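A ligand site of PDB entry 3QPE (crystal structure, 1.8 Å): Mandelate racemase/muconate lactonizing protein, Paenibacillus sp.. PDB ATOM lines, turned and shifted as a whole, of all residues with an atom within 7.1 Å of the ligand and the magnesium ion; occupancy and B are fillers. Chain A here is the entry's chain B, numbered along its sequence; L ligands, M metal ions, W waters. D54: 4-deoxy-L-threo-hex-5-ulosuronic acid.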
ATOM      1  N   ALA A  32     -25.955  -5.991   9.296  1.00  0.00           N
ATOM      2  CA  ALA A  32     -24.547  -5.727   8.996  1.00  0.00           C
ATOM      3  C   ALA A  32     -23.682  -5.827  10.255  1.00  0.00           C
ATOM      4  O   ALA A  32     -24.204  -5.913  11.363  1.00  0.00           O
ATOM      5  CB  ALA A  32     -24.401  -4.346   8.368  1.00  0.00           C
ATOM      6  N   ASN A  33     -22.367  -5.832  10.062  1.00  0.00           N
ATOM      7  CA  ASN A  33     -21.435  -5.644  11.153  1.00  0.00           C
ATOM      8  C   ASN A  33     -20.481  -4.488  10.817  1.00  0.00           C
ATOM      9  O   ASN A  33     -20.686  -3.783   9.834  1.00  0.00           O
ATOM     10  CB  ASN A  33     -20.691  -6.950  11.522  1.00  0.00           C
ATOM     11  CG  ASN A  33     -19.611  -7.341  10.519  1.00  0.00           C
ATOM     12  OD1 ASN A  33     -19.260  -6.577   9.619  1.00  0.00           O
ATOM     13  ND2 ASN A  33     -19.089  -8.564  10.670  1.00  0.00           N
ATOM     14  N   GLY A  34     -19.467  -4.282  11.640  1.00  0.00           N
ATOM     15  CA  GLY A  34     -18.559  -3.174  11.425  1.00  0.00           C
ATOM     16  C   GLY A  34     -17.998  -3.062  10.019  1.00  0.00           C
ATOM     17  O   GLY A  34     -17.835  -1.962   9.500  1.00  0.00           O
ATOM     18  N   ARG A  35     -17.682  -4.203   9.400  1.00  0.00           N
ATOM     19  CA  ARG A  35     -16.946  -4.184   8.142  1.00  0.00           C
ATOM     20  C   ARG A  35     -17.754  -4.575   6.894  1.00  0.00           C
ATOM     21  O   ARG A  35     -17.412  -4.163   5.795  1.00  0.00           O
ATOM     22  CB  ARG A  35     -15.683  -5.046   8.239  1.00  0.00           C
ATOM     23  CG  ARG A  35     -15.953  -6.511   8.612  1.00  0.00           C
ATOM     24  CD  ARG A  35     -14.675  -7.329   8.568  1.00  0.00           C
ATOM     25  NE  ARG A  35     -14.169  -7.434   7.200  1.00  0.00           N
ATOM     26  CZ  ARG A  35     -14.585  -8.337   6.307  1.00  0.00           C
ATOM     27  NH1 ARG A  35     -14.067  -8.346   5.096  1.00  0.00           N
ATOM     28  NH2 ARG A  35     -15.536  -9.204   6.630  1.00  0.00           N
ATOM     29  N   ILE A  36     -18.822  -5.359   7.069  1.00  0.00           N
ATOM     30  CA  ILE A  36     -19.612  -5.813   5.913  1.00  0.00           C
ATOM     31  C   ILE A  36     -21.131  -5.725   6.091  1.00  0.00           C
ATOM     32  O   ILE A  36     -21.634  -5.354   7.159  1.00  0.00           O
ATOM     33  CB  ILE A  36     -19.235  -7.243   5.460  1.00  0.00           C
ATOM     34  CG1 ILE A  36     -19.511  -8.274   6.569  1.00  0.00           C
ATOM     35  CG2 ILE A  36     -17.771  -7.319   5.045  1.00  0.00           C
ATOM     36  CD1 ILE A  36     -19.209  -9.728   6.141  1.00  0.00           C
ATOM     37  N   GLY A  37     -21.864  -6.070   5.036  1.00  0.00           N
ATOM     38  CA  GLY A  37     -23.300  -5.872   5.005  1.00  0.00           C
ATOM     39  C   GLY A  37     -24.112  -6.942   5.705  1.00  0.00           C
ATOM     40  O   GLY A  37     -23.587  -7.754   6.453  1.00  0.00           O
ATOM     41  N   HIS A  39     -25.953 -10.057   6.954  1.00  0.00           N
ATOM     42  CA  HIS A  39     -25.561 -11.466   6.946  1.00  0.00           C
ATOM     43  C   HIS A  39     -26.717 -12.386   6.619  1.00  0.00           C
ATOM     44  O   HIS A  39     -26.511 -13.489   6.133  1.00  0.00           O
ATOM     45  CB  HIS A  39     -24.963 -11.835   8.293  1.00  0.00           C
ATOM     46  CG  HIS A  39     -23.622 -11.222   8.533  1.00  0.00           C
ATOM     47  ND1 HIS A  39     -23.441  -9.862   8.611  1.00  0.00           N
ATOM     48  CD2 HIS A  39     -22.402 -11.778   8.659  1.00  0.00           C
ATOM     49  CE1 HIS A  39     -22.156  -9.606   8.806  1.00  0.00           C
ATOM     50  NE2 HIS A  39     -21.502 -10.757   8.841  1.00  0.00           N
ATOM     51  N   TYR A 131     -22.820 -17.512  25.054  1.00  0.00           N
ATOM     52  CA  TYR A 131     -23.331 -16.157  24.870  1.00  0.00           C
ATOM     53  C   TYR A 131     -24.109 -16.019  23.570  1.00  0.00           C
ATOM     54  O   TYR A 131     -23.830 -16.715  22.599  1.00  0.00           O
ATOM     55  CB  TYR A 131     -22.208 -15.103  24.931  1.00  0.00           C
ATOM     56  CG  TYR A 131     -21.177 -15.154  23.815  1.00  0.00           C
ATOM     57  CD1 TYR A 131     -21.406 -14.541  22.588  1.00  0.00           C
ATOM     58  CD2 TYR A 131     -19.949 -15.769  24.017  1.00  0.00           C
ATOM     59  CE1 TYR A 131     -20.439 -14.565  21.575  1.00  0.00           C
ATOM     60  CE2 TYR A 131     -18.993 -15.806  23.019  1.00  0.00           C
ATOM     61  CZ  TYR A 131     -19.233 -15.206  21.806  1.00  0.00           C
ATOM     62  OH  TYR A 131     -18.254 -15.243  20.830  1.00  0.00           O
ATOM     63  N   THR A 133     -24.728 -14.393  20.362  1.00  0.00           N
ATOM     64  CA  THR A 133     -23.865 -13.618  19.453  1.00  0.00           C
ATOM     65  C   THR A 133     -24.655 -12.894  18.352  1.00  0.00           C
ATOM     66  O   THR A 133     -24.064 -12.319  17.444  1.00  0.00           O
ATOM     67  CB  THR A 133     -22.839 -14.521  18.779  1.00  0.00           C
ATOM     68  OG1 THR A 133     -21.744 -13.734  18.270  1.00  0.00           O
ATOM     69  CG2 THR A 133     -23.491 -15.292  17.654  1.00  0.00           C
ATOM     70  N   TYR A 136     -26.605  -7.848  15.908  1.00  0.00           N
ATOM     71  CA  TYR A 136     -25.897  -7.183  14.813  1.00  0.00           C
ATOM     72  C   TYR A 136     -26.407  -5.756  14.657  1.00  0.00           C
ATOM     73  O   TYR A 136     -27.175  -5.267  15.493  1.00  0.00           O
ATOM     74  CB  TYR A 136     -26.039  -7.997  13.524  1.00  0.00           C
ATOM     75  CG  TYR A 136     -25.002  -9.093  13.399  1.00  0.00           C
ATOM     76  CD1 TYR A 136     -24.966 -10.156  14.308  1.00  0.00           C
ATOM     77  CD2 TYR A 136     -24.047  -9.076  12.391  1.00  0.00           C
ATOM     78  CE1 TYR A 136     -23.990 -11.169  14.202  1.00  0.00           C
ATOM     79  CE2 TYR A 136     -23.088 -10.069  12.277  1.00  0.00           C
ATOM     80  CZ  TYR A 136     -23.061 -11.116  13.195  1.00  0.00           C
ATOM     81  OH  TYR A 136     -22.098 -12.094  13.082  1.00  0.00           O
ATOM     82  N   LYS A 168     -23.067 -10.810  23.158  1.00  0.00           N
ATOM     83  CA  LYS A 168     -22.063 -10.074  22.406  1.00  0.00           C
ATOM     84  C   LYS A 168     -22.734  -9.112  21.426  1.00  0.00           C
ATOM     85  O   LYS A 168     -23.560  -9.515  20.610  1.00  0.00           O
ATOM     86  CB  LYS A 168     -21.087 -10.994  21.674  1.00  0.00           C
ATOM     87  CG  LYS A 168     -19.852 -10.264  21.165  1.00  0.00           C
ATOM     88  CD  LYS A 168     -18.723 -11.210  20.763  1.00  0.00           C
ATOM     89  CE  LYS A 168     -19.041 -11.950  19.477  1.00  0.00           C
ATOM     90  NZ  LYS A 168     -17.985 -12.941  19.166  1.00  0.00           N
ATOM     91  N   LYS A 170     -22.474  -6.269  18.424  1.00  0.00           N
ATOM     92  CA  LYS A 170     -21.655  -5.712  17.357  1.00  0.00           C
ATOM     93  C   LYS A 170     -21.591  -4.204  17.491  1.00  0.00           C
ATOM     94  O   LYS A 170     -22.609  -3.539  17.665  1.00  0.00           O
ATOM     95  CB  LYS A 170     -22.211  -6.110  15.997  1.00  0.00           C
ATOM     96  CG  LYS A 170     -22.156  -7.596  15.692  1.00  0.00           C
ATOM     97  CD  LYS A 170     -20.728  -8.081  15.539  1.00  0.00           C
ATOM     98  CE  LYS A 170     -20.702  -9.581  15.235  1.00  0.00           C
ATOM     99  NZ  LYS A 170     -19.324 -10.127  15.108  1.00  0.00           N
ATOM    100  N   ASP A 207     -17.852  -6.355  19.938  1.00  0.00           N
ATOM    101  CA  ASP A 207     -17.029  -6.779  18.814  1.00  0.00           C
ATOM    102  C   ASP A 207     -17.117  -5.708  17.725  1.00  0.00           C
ATOM    103  O   ASP A 207     -18.186  -5.476  17.183  1.00  0.00           O
ATOM    104  CB  ASP A 207     -17.573  -8.110  18.303  1.00  0.00           C
ATOM    105  CG  ASP A 207     -16.756  -8.694  17.179  1.00  0.00           C
ATOM    106  OD1 ASP A 207     -15.841  -8.030  16.650  1.00  0.00           O
ATOM    107  OD2 ASP A 207     -17.066  -9.845  16.790  1.00  0.00           O
ATOM    108  N   ALA A 208     -15.994  -5.070  17.411  1.00  0.00           N
ATOM    109  CA  ALA A 208     -15.961  -3.971  16.447  1.00  0.00           C
ATOM    110  C   ALA A 208     -15.697  -4.429  15.025  1.00  0.00           C
ATOM    111  O   ALA A 208     -15.779  -3.624  14.102  1.00  0.00           O
ATOM    112  CB  ALA A 208     -14.903  -2.962  16.842  1.00  0.00           C
ATOM    113  N   ASN A 209     -15.353  -5.709  14.864  1.00  0.00           N
ATOM    114  CA  ASN A 209     -14.913  -6.214  13.575  1.00  0.00           C
ATOM    115  C   ASN A 209     -13.906  -5.265  12.933  1.00  0.00           C
ATOM    116  O   ASN A 209     -14.001  -4.940  11.746  1.00  0.00           O
ATOM    117  CB  ASN A 209     -16.090  -6.520  12.656  1.00  0.00           C
ATOM    118  CG  ASN A 209     -16.810  -7.787  13.065  1.00  0.00           C
ATOM    119  OD1 ASN A 209     -17.861  -7.739  13.696  1.00  0.00           O
ATOM    120  ND2 ASN A 209     -16.222  -8.934  12.726  1.00  0.00           N
ATOM    121  N   GLU A 233     -13.533  -7.328  21.549  1.00  0.00           N
ATOM    122  CA  GLU A 233     -13.157  -8.223  20.485  1.00  0.00           C
ATOM    123  C   GLU A 233     -12.831  -7.438  19.215  1.00  0.00           C
ATOM    124  O   GLU A 233     -13.642  -6.631  18.761  1.00  0.00           O
ATOM    125  CB  GLU A 233     -14.310  -9.215  20.232  1.00  0.00           C
ATOM    126  CG  GLU A 233     -14.066 -10.184  19.096  1.00  0.00           C
ATOM    127  CD  GLU A 233     -15.026 -11.360  19.135  1.00  0.00           C
ATOM    128  OE1 GLU A 233     -15.649 -11.610  20.188  1.00  0.00           O
ATOM    129  OE2 GLU A 233     -15.162 -12.062  18.107  1.00  0.00           O
ATOM    130  N   GLU A 234     -11.647  -7.651  18.668  1.00  0.00           N
ATOM    131  CA  GLU A 234     -11.240  -7.011  17.422  1.00  0.00           C
ATOM    132  C   GLU A 234     -11.577  -5.521  17.323  1.00  0.00           C
ATOM    133  O   GLU A 234     -12.302  -5.083  16.434  1.00  0.00           O
ATOM    134  CB  GLU A 234     -11.864  -7.763  16.238  1.00  0.00           C
ATOM    135  CG  GLU A 234     -11.441  -9.221  16.164  1.00  0.00           C
ATOM    136  CD  GLU A 234     -11.417  -9.756  14.743  1.00  0.00           C
ATOM    137  OE1 GLU A 234     -12.474  -9.845  14.103  1.00  0.00           O
ATOM    138  OE2 GLU A 234     -10.338 -10.082  14.252  1.00  0.00           O
ATOM    139  N   GLU A 263      -9.857 -14.459  15.089  1.00  0.00           N
ATOM    140  CA  GLU A 263     -10.592 -15.011  13.936  1.00  0.00           C
ATOM    141  C   GLU A 263     -10.022 -14.509  12.609  1.00  0.00           C
ATOM    142  O   GLU A 263      -9.146 -13.628  12.593  1.00  0.00           O
ATOM    143  CB  GLU A 263     -12.081 -14.637  14.038  1.00  0.00           C
ATOM    144  CG  GLU A 263     -12.359 -13.177  13.721  1.00  0.00           C
ATOM    145  CD  GLU A 263     -13.791 -12.782  13.996  1.00  0.00           C
ATOM    146  OE1 GLU A 263     -14.460 -12.284  13.065  1.00  0.00           O
ATOM    147  OE2 GLU A 263     -14.239 -12.973  15.140  1.00  0.00           O
ATOM    148  N   GLN A 283      -9.293 -16.576  19.624  1.00  0.00           N
ATOM    149  CA  GLN A 283     -10.571 -16.914  19.027  1.00  0.00           C
ATOM    150  C   GLN A 283     -10.518 -17.525  17.617  1.00  0.00           C
ATOM    151  O   GLN A 283     -11.398 -17.283  16.803  1.00  0.00           O
ATOM    152  CB  GLN A 283     -11.471 -15.671  19.016  1.00  0.00           C
ATOM    153  CG  GLN A 283     -11.537 -14.955  20.353  1.00  0.00           C
ATOM    154  CD  GLN A 283     -12.402 -13.731  20.269  1.00  0.00           C
ATOM    155  OE1 GLN A 283     -12.048 -12.744  19.624  1.00  0.00           O
ATOM    156  NE2 GLN A 283     -13.571 -13.795  20.893  1.00  0.00           N
ATOM    157  N   HIS A 311     -14.018 -18.987  17.801  1.00  0.00           N
ATOM    158  CA  HIS A 311     -15.005 -18.321  16.964  1.00  0.00           C
ATOM    159  C   HIS A 311     -15.938 -19.348  16.316  1.00  0.00           C
ATOM    160  O   HIS A 311     -15.496 -20.420  15.867  1.00  0.00           O
ATOM    161  CB  HIS A 311     -14.287 -17.476  15.909  1.00  0.00           C
ATOM    162  CG  HIS A 311     -15.194 -16.934  14.842  1.00  0.00           C
ATOM    163  ND1 HIS A 311     -15.503 -17.651  13.710  1.00  0.00           N
ATOM    164  CD2 HIS A 311     -15.827 -15.748  14.734  1.00  0.00           C
ATOM    165  CE1 HIS A 311     -16.307 -16.926  12.948  1.00  0.00           C
ATOM    166  NE2 HIS A 311     -16.520 -15.763  13.547  1.00  0.00           N
ATOM    167  N   CYS A 312     -17.218 -19.028  16.308  1.00  0.00           N
ATOM    168  CA  CYS A 312     -18.194 -19.797  15.548  1.00  0.00           C
ATOM    169  C   CYS A 312     -19.289 -18.880  15.049  1.00  0.00           C
ATOM    170  O   CYS A 312     -20.100 -18.367  15.821  1.00  0.00           O
ATOM    171  CB  CYS A 312     -18.812 -20.920  16.383  1.00  0.00           C
ATOM    172  SG  CYS A 312     -19.924 -21.998  15.436  1.00  0.00           S
ATOM    173  N   TYR A 313     -19.303 -18.673  13.738  1.00  0.00           N
ATOM    174  CA  TYR A 313     -20.414 -17.978  13.111  1.00  0.00           C
ATOM    175  C   TYR A 313     -20.504 -18.394  11.643  1.00  0.00           C
ATOM    176  O   TYR A 313     -19.487 -18.449  10.947  1.00  0.00           O
ATOM    177  CB  TYR A 313     -20.291 -16.451  13.264  1.00  0.00           C
ATOM    178  CG  TYR A 313     -21.580 -15.764  12.938  1.00  0.00           C
ATOM    179  CD1 TYR A 313     -22.554 -15.571  13.902  1.00  0.00           C
ATOM    180  CD2 TYR A 313     -21.846 -15.327  11.641  1.00  0.00           C
ATOM    181  CE1 TYR A 313     -23.750 -14.950  13.601  1.00  0.00           C
ATOM    182  CE2 TYR A 313     -23.042 -14.706  11.340  1.00  0.00           C
ATOM    183  CZ  TYR A 313     -23.978 -14.526  12.314  1.00  0.00           C
ATOM    184  OH  TYR A 313     -25.154 -13.924  11.997  1.00  0.00           O
ATOM    185  N   GLY A 314     -21.716 -18.703  11.192  1.00  0.00           N
ATOM    186  CA  GLY A 314     -21.943 -19.077   9.801  1.00  0.00           C
ATOM    187  C   GLY A 314     -21.924 -20.583   9.595  1.00  0.00           C
ATOM    188  O   GLY A 314     -22.114 -21.100   8.491  1.00  0.00           O
ATOM    189  N   GLU A 336     -19.935 -19.795  21.490  1.00  0.00           N
ATOM    190  CA  GLU A 336     -20.571 -18.707  20.744  1.00  0.00           C
ATOM    191  C   GLU A 336     -21.842 -19.196  20.070  1.00  0.00           C
ATOM    192  O   GLU A 336     -21.801 -19.994  19.129  1.00  0.00           O
ATOM    193  CB  GLU A 336     -19.610 -18.092  19.716  1.00  0.00           C
ATOM    194  CG  GLU A 336     -20.184 -16.876  18.990  1.00  0.00           C
ATOM    195  CD  GLU A 336     -19.186 -16.192  18.075  1.00  0.00           C
ATOM    196  OE1 GLU A 336     -18.054 -16.699  17.910  1.00  0.00           O
ATOM    197  OE2 GLU A 336     -19.534 -15.136  17.509  1.00  0.00           O
HETATM  198  OAA D54 L   1     -18.415 -14.618   9.197  1.00  0.00           O
HETATM  199  OAB D54 L   1     -18.873 -11.627   9.268  1.00  0.00           O
HETATM  200  OAC D54 L   1     -16.822 -11.639  14.068  1.00  0.00           O
HETATM  201  OAD D54 L   1     -17.442 -13.067  16.388  1.00  0.00           O
HETATM  202  CAE D54 L   1     -18.125 -13.796  10.084  1.00  0.00           C
HETATM  203  CAF D54 L   1     -19.009 -12.563  10.344  1.00  0.00           C
HETATM  204  CAG D54 L   1     -18.576 -11.952  11.697  1.00  0.00           C
HETATM  205  CAH D54 L   1     -18.193 -13.065  12.689  1.00  0.00           C
HETATM  206  CAI D54 L   1     -17.608 -12.594  14.026  1.00  0.00           C
HETATM  207  CAJ D54 L   1     -18.009 -13.365  15.319  1.00  0.00           C
HETATM  208  OAK D54 L   1     -19.650 -11.157  12.231  1.00  0.00           O
HETATM  209  OAL D54 L   1     -18.875 -14.276  15.216  1.00  0.00           O
HETATM  210 MG    MG M   1     -15.686 -11.502  16.103  1.00  0.00          MG
HETATM  211  O   HOH W   1     -14.376  -9.878  15.512  1.00  0.00           O
HETATM  212  O   HOH W   2     -16.780  -9.985   9.186  1.00  0.00           O
HETATM  213  O   HOH W   3     -21.196 -12.992  15.728  1.00  0.00           O
HETATM  214  O   HOH W   4     -17.499 -16.808  10.016  1.00  0.00           O
HETATM  215  O   HOH W   5     -15.580 -14.956  18.424  1.00  0.00           O
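CD1 of Ile 36 touches OAB of the ligand, 3.7 Å away. Tyr 313 touches the ligand (CB to OAL, 3.2 Å). 13 residues have an atom within 4 Å of the ligand: Asn 33, Ile 36, His 39, Tyr 136, Lys 168, Lys 170, Asp 207, Asn 209, Glu 233, Glu 263, His 311, Tyr 313 and Glu 336. The nearest printed residue that does not touch the ligand is Thr 133 (4.2 Å).
Of the 24 residues printed, 3 come within 4 Å of the magnesium ion.
The magnesium ion is bound by OE2 of Glu 233 (2.1 Å), water W1 (2.2 Å), OD2 of Asp 207 (2.3 Å), OE2 of Glu 263 (2.3 Å), OAC of the ligand (2.3 Å) and OAD of the ligand (2.4 Å).
Water W1 lies within hydrogen-bond range of the side-chain carboxylate of Asp 207 (2.6 Å), the side-chain carboxylate of Glu 263 (3.4 Å) and the side-chain amide nitrogen of Asn 209 (3.5 Å). Water W4 bridges OAA of the ligand and O of Tyr 313. Water W2 lies within hydrogen-bond range of an oxygen (OAB) of the ligand (2.7 Å), the guanidinium group of Arg 35 (2.9 Å) and the side-chain amide nitrogen of Asn 33 (3.1 Å). Water W3 lies within hydrogen-bond range of an oxygen (OAL) of the ligand (2.7 Å), the side-chain hydroxyl of Thr 133 (2.7 Å), the side-chain hydroxyl of Tyr 136 (2.9 Å), the side-chain carboxylate of Glu 336 (3.2 Å) and the side-chain amino group of Lys 170 (3.5 Å). Water W5 lies within hydrogen-bond range of the side-chain carboxylate of Glu 336 (3.1 Å), the side-chain amino group of Lys 168 (3.2 Å) and the side-chain amide nitrogen of Gln 283 (3.4 Å).
The side-chain carboxylate (OE1) of Glu 233 is in hydrogen-bond range of the side-chain amide nitrogen (NE2) of Gln 283 (3.1 Å). The side-chain carboxylate (OD1) of Asp 207 is in hydrogen-bond range of the backbone NH (N) of Asn 209 (3.0 Å). The side-chain amino group (NZ) of Lys 168 is in salt-bridge range of the side-chain carboxylate (OE2) of Glu 336. The side-chain carboxylate of Glu 336 is in hydrogen-bond range of the side-chain hydroxyl of Thr 133, 2.7 Å away. NZ of Lys 168 is in hydrogen-bond range of OH of Tyr 131, at 2.9 Å. The side-chain amide nitrogen (ND2) of Asn 33 is in hydrogen-bond range of the side-chain amide oxygen (OD1) of Asn 209 (3.4 Å). N of Asn 209 lies within hydrogen-bond range of O of Glu 234, 3.5 Å away. N of His 311 sits close to O of Gln 283, 3.3 Å away.
OE2 of Glu 336 lies close to OAL of the ligand, at 2.5 Å. OH of Tyr 136 lies within hydrogen-bond range of OAK of the ligand, at 2.8 Å. A ring nitrogen (NE2) of His 39 is in hydrogen-bond range of an oxygen (OAB) of the ligand. An oxygen (OAD) of the ligand lies close to the side-chain amino group of Lys 168 (2.8 Å). NZ of Lys 170 is in hydrogen-bond range of OAK of the ligand, at 3.1 Å. The side-chain amide nitrogen (ND2) of Asn 33 sits at hydrogen-bond distance from an oxygen (OAK) of the ligand (3.1 Å). The side-chain amide nitrogen (ND2) of Asn 209 sits close to an oxygen (OAC) of the ligand (3.1 Å). A ring nitrogen (NE2) of His 311 sits at hydrogen-bond distance from an oxygen (OAL) of the ligand, at 3.2 Å.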
